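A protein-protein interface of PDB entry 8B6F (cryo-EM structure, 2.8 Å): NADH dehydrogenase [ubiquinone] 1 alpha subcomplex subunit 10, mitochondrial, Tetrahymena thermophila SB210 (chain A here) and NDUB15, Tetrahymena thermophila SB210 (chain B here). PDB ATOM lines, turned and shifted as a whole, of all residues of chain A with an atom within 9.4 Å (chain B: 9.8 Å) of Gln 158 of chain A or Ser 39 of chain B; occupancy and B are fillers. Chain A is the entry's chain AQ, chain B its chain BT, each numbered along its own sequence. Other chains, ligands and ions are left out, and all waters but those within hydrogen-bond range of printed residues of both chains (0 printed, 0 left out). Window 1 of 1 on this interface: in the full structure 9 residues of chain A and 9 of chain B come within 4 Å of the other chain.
O of Pro 157 of chain A is in hydrogen-bond range of N of Gly 40 of chain B (3.5 Å).
The backbone carbonyl oxygen (O) of Gln 158 of chain A sits at hydrogen-bond distance from the backbone NH (N) of Ser 39 of chain B (2.7 Å).
Of the 13 printed residues of chain A, 5 touch a printed residue of chain B.
Printed residues of chain B that touch a printed residue of chain A: Ala 37, Leu 38, Ser 39, Gly 40, Phe 41 and Arg 42.
Hydrophobic or aromatic side chains of chain B that line the printed part of chain A: Ala 37, Leu 38 and Phe 41.
Along chain B the printed residues that touch a printed residue of chain A span positions 37 to 42.
Among the printed residues, 11 pairs touch across the chains.
Ser 39 of chain B touches just one residue of chain A: Gln 158 (2.7 Å).
Printed residues of chain B within 4 Å of Pro 157 of chain A: Ala 37 and Gly 40.
Of chain A, only Tyr 156 (3.6 Å), Pro 157 (3.5 Å) and Gln 158 (3.8 Å) come within 4 Å of Gly 40 of chain B.
Of the printed residues of chain B, Phe 130 of chain A touches Arg 42 (3.5 Å).
Of the printed residues of chain A, Ala 37 of chain B touches Tyr 156 (3.7 Å), Pro 157 (3.9 Å) and Asp 160 (3.5 Å).
Of the printed residues of chain A, Phe 41 of chain B touches Tyr 156 (3.7 Å).
Printed residues of chain B within 4 Å of Tyr 156 of chain A: Ala 37 (3.7 Å), Gly 40 (3.6 Å) and Phe 41 (3.7 Å).
Printed residues of chain A within 4 Å of Arg 42 of chain B: Phe 130.
Pro 132 of chain A touches none of the printed residues of chain B.
Phe 133 of chain A touches none of the printed residues of chain B.
The nearest residue of chain B that does not touch Gln 158 of chain A is Arg 42 of chain B (4.3 Å).
The nearest residue of chain A that does not touch Ser 39 of chain B is Pro 157 of chain A (4.2 Å).
Among the printed residues, merely in contact across the chains: Asp 160 of chain A with Leu 38 of chain B, Phe 130 of chain A with Arg 42 of chain B, Asp 160 of chain A with Ala 37 of chain B, Gln 158 of chain A with Leu 38 of chain B, Tyr 156 of chain A with Gly 40 of chain B, Tyr 156 of chain A with Ala 37 of chain B, Tyr 156 of chain A with Phe 41 of chain B, Gln 158 of chain A with Gly 40 of chain B and Pro 157 of chain A with Ala 37 of chain B.
The backbone carbonyl oxygen (O) of Ser 39 of chain B lies within hydrogen-bond range of the guanidinium group (NE) of Arg 42 of chain B (3.2 Å).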
ATOM      1  N   PHE A 130     -17.326 -17.464   0.013  1.00  0.00           N
ATOM      2  CA  PHE A 130     -15.992 -17.091   0.467  1.00  0.00           C
ATOM      3  C   PHE A 130     -15.771 -17.509   1.912  1.00  0.00           C
ATOM      4  O   PHE A 130     -16.517 -17.112   2.809  1.00  0.00           O
ATOM      5  CB  PHE A 130     -15.799 -15.582   0.311  1.00  0.00           C
ATOM      6  CG  PHE A 130     -14.415 -15.119   0.644  1.00  0.00           C
ATOM      7  CD1 PHE A 130     -13.350 -15.438  -0.179  1.00  0.00           C
ATOM      8  CD2 PHE A 130     -14.180 -14.354   1.769  1.00  0.00           C
ATOM      9  CE1 PHE A 130     -12.073 -15.011   0.122  1.00  0.00           C
ATOM     10  CE2 PHE A 130     -12.907 -13.923   2.074  1.00  0.00           C
ATOM     11  CZ  PHE A 130     -11.852 -14.252   1.250  1.00  0.00           C
ATOM     12  N   ASP A 131     -14.738 -18.319   2.128  1.00  0.00           N
ATOM     13  CA  ASP A 131     -14.382 -18.804   3.453  1.00  0.00           C
ATOM     14  C   ASP A 131     -12.941 -19.299   3.437  1.00  0.00           C
ATOM     15  O   ASP A 131     -12.704 -20.512   3.375  1.00  0.00           O
ATOM     16  CB  ASP A 131     -15.331 -19.921   3.887  1.00  0.00           C
ATOM     17  CG  ASP A 131     -15.071 -20.388   5.302  1.00  0.00           C
ATOM     18  OD1 ASP A 131     -14.336 -19.693   6.034  1.00  0.00           O
ATOM     19  OD2 ASP A 131     -15.596 -21.453   5.683  1.00  0.00           O
ATOM     20  N   PRO A 132     -11.954 -18.401   3.488  1.00  0.00           N
ATOM     21  CA  PRO A 132     -10.559 -18.854   3.374  1.00  0.00           C
ATOM     22  C   PRO A 132     -10.142 -19.809   4.472  1.00  0.00           C
ATOM     23  O   PRO A 132      -9.297 -20.681   4.236  1.00  0.00           O
ATOM     24  CB  PRO A 132      -9.761 -17.544   3.426  1.00  0.00           C
ATOM     25  CG  PRO A 132     -10.649 -16.579   4.105  1.00  0.00           C
ATOM     26  CD  PRO A 132     -12.052 -16.959   3.760  1.00  0.00           C
ATOM     27  N   PHE A 133     -10.701 -19.671   5.666  1.00  0.00           N
ATOM     28  CA  PHE A 133     -10.409 -20.580   6.761  1.00  0.00           C
ATOM     29  C   PHE A 133     -11.463 -21.682   6.798  1.00  0.00           C
ATOM     30  O   PHE A 133     -12.540 -21.564   6.210  1.00  0.00           O
ATOM     31  CB  PHE A 133     -10.356 -19.819   8.086  1.00  0.00           C
ATOM     32  CG  PHE A 133      -9.627 -18.506   7.997  1.00  0.00           C
ATOM     33  CD1 PHE A 133      -8.520 -18.363   7.176  1.00  0.00           C
ATOM     34  CD2 PHE A 133     -10.059 -17.409   8.721  1.00  0.00           C
ATOM     35  CE1 PHE A 133      -7.856 -17.154   7.087  1.00  0.00           C
ATOM     36  CE2 PHE A 133      -9.400 -16.199   8.636  1.00  0.00           C
ATOM     37  CZ  PHE A 133      -8.297 -16.070   7.819  1.00  0.00           C
ATOM     38  N   LYS A 139     -11.585 -26.834   4.842  1.00  0.00           N
ATOM     39  CA  LYS A 139     -10.385 -26.370   4.158  1.00  0.00           C
ATOM     40  C   LYS A 139      -9.397 -27.523   4.052  1.00  0.00           C
ATOM     41  O   LYS A 139      -9.003 -28.103   5.069  1.00  0.00           O
ATOM     42  CB  LYS A 139      -9.762 -25.193   4.910  1.00  0.00           C
ATOM     43  CG  LYS A 139      -8.525 -24.596   4.257  1.00  0.00           C
ATOM     44  CD  LYS A 139      -8.871 -23.892   2.960  1.00  0.00           C
ATOM     45  CE  LYS A 139      -7.656 -23.198   2.366  1.00  0.00           C
ATOM     46  NZ  LYS A 139      -7.109 -22.144   3.266  1.00  0.00           N
ATOM     47  N   GLU A 143      -3.879 -26.668   0.068  1.00  0.00           N
ATOM     48  CA  GLU A 143      -4.744 -25.494   0.041  1.00  0.00           C
ATOM     49  C   GLU A 143      -5.765 -25.558  -1.088  1.00  0.00           C
ATOM     50  O   GLU A 143      -6.934 -25.204  -0.898  1.00  0.00           O
ATOM     51  CB  GLU A 143      -3.895 -24.229  -0.085  1.00  0.00           C
ATOM     52  CG  GLU A 143      -2.959 -23.999   1.088  1.00  0.00           C
ATOM     53  CD  GLU A 143      -2.206 -22.690   0.973  1.00  0.00           C
ATOM     54  OE1 GLU A 143      -2.257 -22.070  -0.109  1.00  0.00           O
ATOM     55  OE2 GLU A 143      -1.567 -22.277   1.964  1.00  0.00           O
ATOM     56  N   ASP A 155      -2.124 -21.524  -2.371  1.00  0.00           N
ATOM     57  CA  ASP A 155      -2.904 -20.306  -2.512  1.00  0.00           C
ATOM     58  C   ASP A 155      -2.269 -19.176  -1.709  1.00  0.00           C
ATOM     59  O   ASP A 155      -1.675 -19.393  -0.651  1.00  0.00           O
ATOM     60  CB  ASP A 155      -4.343 -20.525  -2.044  1.00  0.00           C
ATOM     61  CG  ASP A 155      -5.128 -21.428  -2.972  1.00  0.00           C
ATOM     62  OD1 ASP A 155      -4.841 -21.432  -4.188  1.00  0.00           O
ATOM     63  OD2 ASP A 155      -6.037 -22.133  -2.486  1.00  0.00           O
ATOM     64  N   TYR A 156      -2.391 -17.964  -2.228  1.00  0.00           N
ATOM     65  CA  TYR A 156      -1.881 -16.804  -1.512  1.00  0.00           C
ATOM     66  C   TYR A 156      -2.667 -16.624  -0.218  1.00  0.00           C
ATOM     67  O   TYR A 156      -3.903 -16.579  -0.254  1.00  0.00           O
ATOM     68  CB  TYR A 156      -1.984 -15.552  -2.375  1.00  0.00           C
ATOM     69  CG  TYR A 156      -0.801 -15.344  -3.287  1.00  0.00           C
ATOM     70  CD1 TYR A 156       0.330 -14.675  -2.843  1.00  0.00           C
ATOM     71  CD2 TYR A 156      -0.815 -15.814  -4.592  1.00  0.00           C
ATOM     72  CE1 TYR A 156       1.416 -14.480  -3.671  1.00  0.00           C
ATOM     73  CE2 TYR A 156       0.265 -15.624  -5.429  1.00  0.00           C
ATOM     74  CZ  TYR A 156       1.378 -14.955  -4.962  1.00  0.00           C
ATOM     75  OH  TYR A 156       2.458 -14.762  -5.789  1.00  0.00           O
ATOM     76  N   PRO A 157      -2.005 -16.522   0.931  1.00  0.00           N
ATOM     77  CA  PRO A 157      -2.745 -16.373   2.187  1.00  0.00           C
ATOM     78  C   PRO A 157      -3.442 -15.028   2.272  1.00  0.00           C
ATOM     79  O   PRO A 157      -3.038 -14.048   1.641  1.00  0.00           O
ATOM     80  CB  PRO A 157      -1.657 -16.504   3.258  1.00  0.00           C
ATOM     81  CG  PRO A 157      -0.421 -16.053   2.581  1.00  0.00           C
ATOM     82  CD  PRO A 157      -0.548 -16.480   1.147  1.00  0.00           C
ATOM     83  N   GLN A 158      -4.514 -14.992   3.064  1.00  0.00           N
ATOM     84  CA  GLN A 158      -5.226 -13.738   3.281  1.00  0.00           C
ATOM     85  C   GLN A 158      -4.317 -12.705   3.935  1.00  0.00           C
ATOM     86  O   GLN A 158      -4.278 -11.541   3.520  1.00  0.00           O
ATOM     87  CB  GLN A 158      -6.468 -13.985   4.138  1.00  0.00           C
ATOM     88  CG  GLN A 158      -7.487 -14.897   3.482  1.00  0.00           C
ATOM     89  CD  GLN A 158      -8.067 -14.303   2.215  1.00  0.00           C
ATOM     90  OE1 GLN A 158      -8.231 -13.088   2.107  1.00  0.00           O
ATOM     91  NE2 GLN A 158      -8.374 -15.155   1.246  1.00  0.00           N
ATOM     92  N   ASN A 159      -3.570 -13.116   4.953  1.00  0.00           N
ATOM     93  CA  ASN A 159      -2.592 -12.261   5.610  1.00  0.00           C
ATOM     94  C   ASN A 159      -1.208 -12.627   5.090  1.00  0.00           C
ATOM     95  O   ASN A 159      -0.760 -13.765   5.261  1.00  0.00           O
ATOM     96  CB  ASN A 159      -2.663 -12.423   7.127  1.00  0.00           C
ATOM     97  CG  ASN A 159      -1.768 -11.449   7.861  1.00  0.00           C
ATOM     98  OD1 ASN A 159      -1.419 -10.392   7.336  1.00  0.00           O
ATOM     99  ND2 ASN A 159      -1.389 -11.798   9.084  1.00  0.00           N
ATOM    100  N   ASP A 160      -0.535 -11.664   4.460  1.00  0.00           N
ATOM    101  CA  ASP A 160       0.756 -11.895   3.825  1.00  0.00           C
ATOM    102  C   ASP A 160       1.899 -11.243   4.597  1.00  0.00           C
ATOM    103  O   ASP A 160       2.913 -10.862   4.010  1.00  0.00           O
ATOM    104  CB  ASP A 160       0.737 -11.388   2.385  1.00  0.00           C
ATOM    105  CG  ASP A 160       0.597  -9.885   2.301  1.00  0.00           C
ATOM    106  OD1 ASP A 160       0.043  -9.288   3.247  1.00  0.00           O
ATOM    107  OD2 ASP A 160       1.041  -9.301   1.291  1.00  0.00           O
ATOM    108  N   SER A 161       1.747 -11.102   5.911  1.00  0.00           N
ATOM    109  CA  SER A 161       2.808 -10.527   6.722  1.00  0.00           C
ATOM    110  C   SER A 161       4.047 -11.410   6.670  1.00  0.00           C
ATOM    111  O   SER A 161       3.963 -12.636   6.774  1.00  0.00           O
ATOM    112  CB  SER A 161       2.340 -10.356   8.165  1.00  0.00           C
ATOM    113  OG  SER A 161       1.959 -11.599   8.726  1.00  0.00           O
ATOM    114  N   ASP B  36       1.785  -6.660  -4.486  1.00  0.00           N
ATOM    115  CA  ASP B  36       1.064  -6.598  -3.223  1.00  0.00           C
ATOM    116  C   ASP B  36       0.005  -7.694  -3.231  1.00  0.00           C
ATOM    117  O   ASP B  36      -0.868  -7.709  -4.104  1.00  0.00           O
ATOM    118  CB  ASP B  36       0.431  -5.221  -3.034  1.00  0.00           C
ATOM    119  CG  ASP B  36      -0.152  -5.033  -1.654  1.00  0.00           C
ATOM    120  OD1 ASP B  36       0.629  -4.953  -0.683  1.00  0.00           O
ATOM    121  OD2 ASP B  36      -1.394  -4.961  -1.538  1.00  0.00           O
ATOM    122  N   ALA B  37       0.078  -8.602  -2.262  1.00  0.00           N
ATOM    123  CA  ALA B  37      -0.715  -9.826  -2.259  1.00  0.00           C
ATOM    124  C   ALA B  37      -1.503  -9.964  -0.967  1.00  0.00           C
ATOM    125  O   ALA B  37      -1.535 -11.026  -0.342  1.00  0.00           O
ATOM    126  CB  ALA B  37       0.180 -11.042  -2.466  1.00  0.00           C
ATOM    127  N   LEU B  38      -2.159  -8.888  -0.544  1.00  0.00           N
ATOM    128  CA  LEU B  38      -2.974  -8.946   0.658  1.00  0.00           C
ATOM    129  C   LEU B  38      -4.364  -9.472   0.335  1.00  0.00           C
ATOM    130  O   LEU B  38      -4.965  -9.107  -0.679  1.00  0.00           O
ATOM    131  CB  LEU B  38      -3.085  -7.563   1.298  1.00  0.00           C
ATOM    132  CG  LEU B  38      -3.751  -7.521   2.678  1.00  0.00           C
ATOM    133  CD1 LEU B  38      -2.881  -8.194   3.723  1.00  0.00           C
ATOM    134  CD2 LEU B  38      -4.067  -6.091   3.079  1.00  0.00           C
ATOM    135  N   SER B  39      -4.871 -10.337   1.210  1.00  0.00           N
ATOM    136  CA  SER B  39      -6.225 -10.876   1.102  1.00  0.00           C
ATOM    137  C   SER B  39      -6.400 -11.714  -0.165  1.00  0.00           C
ATOM    138  O   SER B  39      -7.368 -11.561  -0.911  1.00  0.00           O
ATOM    139  CB  SER B  39      -7.260  -9.755   1.160  1.00  0.00           C
ATOM    140  OG  SER B  39      -8.562 -10.301   1.137  1.00  0.00           O
ATOM    141  N   GLY B  40      -5.450 -12.613  -0.404  1.00  0.00           N
ATOM    142  CA  GLY B  40      -5.564 -13.579  -1.475  1.00  0.00           C
ATOM    143  C   GLY B  40      -5.036 -13.138  -2.822  1.00  0.00           C
ATOM    144  O   GLY B  40      -5.072 -13.934  -3.769  1.00  0.00           O
ATOM    145  N   PHE B  41      -4.550 -11.905  -2.948  1.00  0.00           N
ATOM    146  CA  PHE B  41      -3.993 -11.407  -4.204  1.00  0.00           C
ATOM    147  C   PHE B  41      -5.026 -11.504  -5.329  1.00  0.00           C
ATOM    148  O   PHE B  41      -4.805 -12.138  -6.363  1.00  0.00           O
ATOM    149  CB  PHE B  41      -2.712 -12.174  -4.560  1.00  0.00           C
ATOM    150  CG  PHE B  41      -1.823 -11.471  -5.557  1.00  0.00           C
ATOM    151  CD1 PHE B  41      -2.293 -10.419  -6.330  1.00  0.00           C
ATOM    152  CD2 PHE B  41      -0.511 -11.876  -5.723  1.00  0.00           C
ATOM    153  CE1 PHE B  41      -1.470  -9.787  -7.239  1.00  0.00           C
ATOM    154  CE2 PHE B  41       0.316 -11.247  -6.631  1.00  0.00           C
ATOM    155  CZ  PHE B  41      -0.165 -10.203  -7.390  1.00  0.00           C
ATOM    156  N   ARG B  42      -6.168 -10.860  -5.109  1.00  0.00           N
ATOM    157  CA  ARG B  42      -7.249 -10.810  -6.085  1.00  0.00           C
ATOM    158  C   ARG B  42      -7.364  -9.386  -6.609  1.00  0.00           C
ATOM    159  O   ARG B  42      -7.623  -8.457  -5.838  1.00  0.00           O
ATOM    160  CB  ARG B  42      -8.566 -11.264  -5.459  1.00  0.00           C
ATOM    161  CG  ARG B  42      -8.563 -12.710  -4.993  1.00  0.00           C
ATOM    162  CD  ARG B  42      -9.801 -13.016  -4.172  1.00  0.00           C
ATOM    163  NE  ARG B  42      -9.801 -12.289  -2.907  1.00  0.00           N
ATOM    164  CZ  ARG B  42     -10.857 -12.159  -2.116  1.00  0.00           C
ATOM    165  NH1 ARG B  42     -12.031 -12.677  -2.437  1.00  0.00           N
ATOM    166  NH2 ARG B  42     -10.734 -11.487  -0.975  1.00  0.00           N
ATOM    167  N   ILE B  43      -7.183  -9.221  -7.917  1.00  0.00           N
ATOM    168  CA  ILE B  43      -7.175  -7.916  -8.566  1.00  0.00           C
ATOM    169  C   ILE B  43      -8.327  -7.876  -9.558  1.00  0.00           C
ATOM    170  O   ILE B  43      -8.474  -8.788 -10.380  1.00  0.00           O
ATOM    171  CB  ILE B  43      -5.839  -7.638  -9.277  1.00  0.00           C
ATOM    172  CG1 ILE B  43      -4.653  -8.014  -8.383  1.00  0.00           C
ATOM    173  CG2 ILE B  43      -5.760  -6.175  -9.692  1.00  0.00           C
ATOM    174  CD1 ILE B  43      -4.524  -7.185  -7.133  1.00  0.00           C
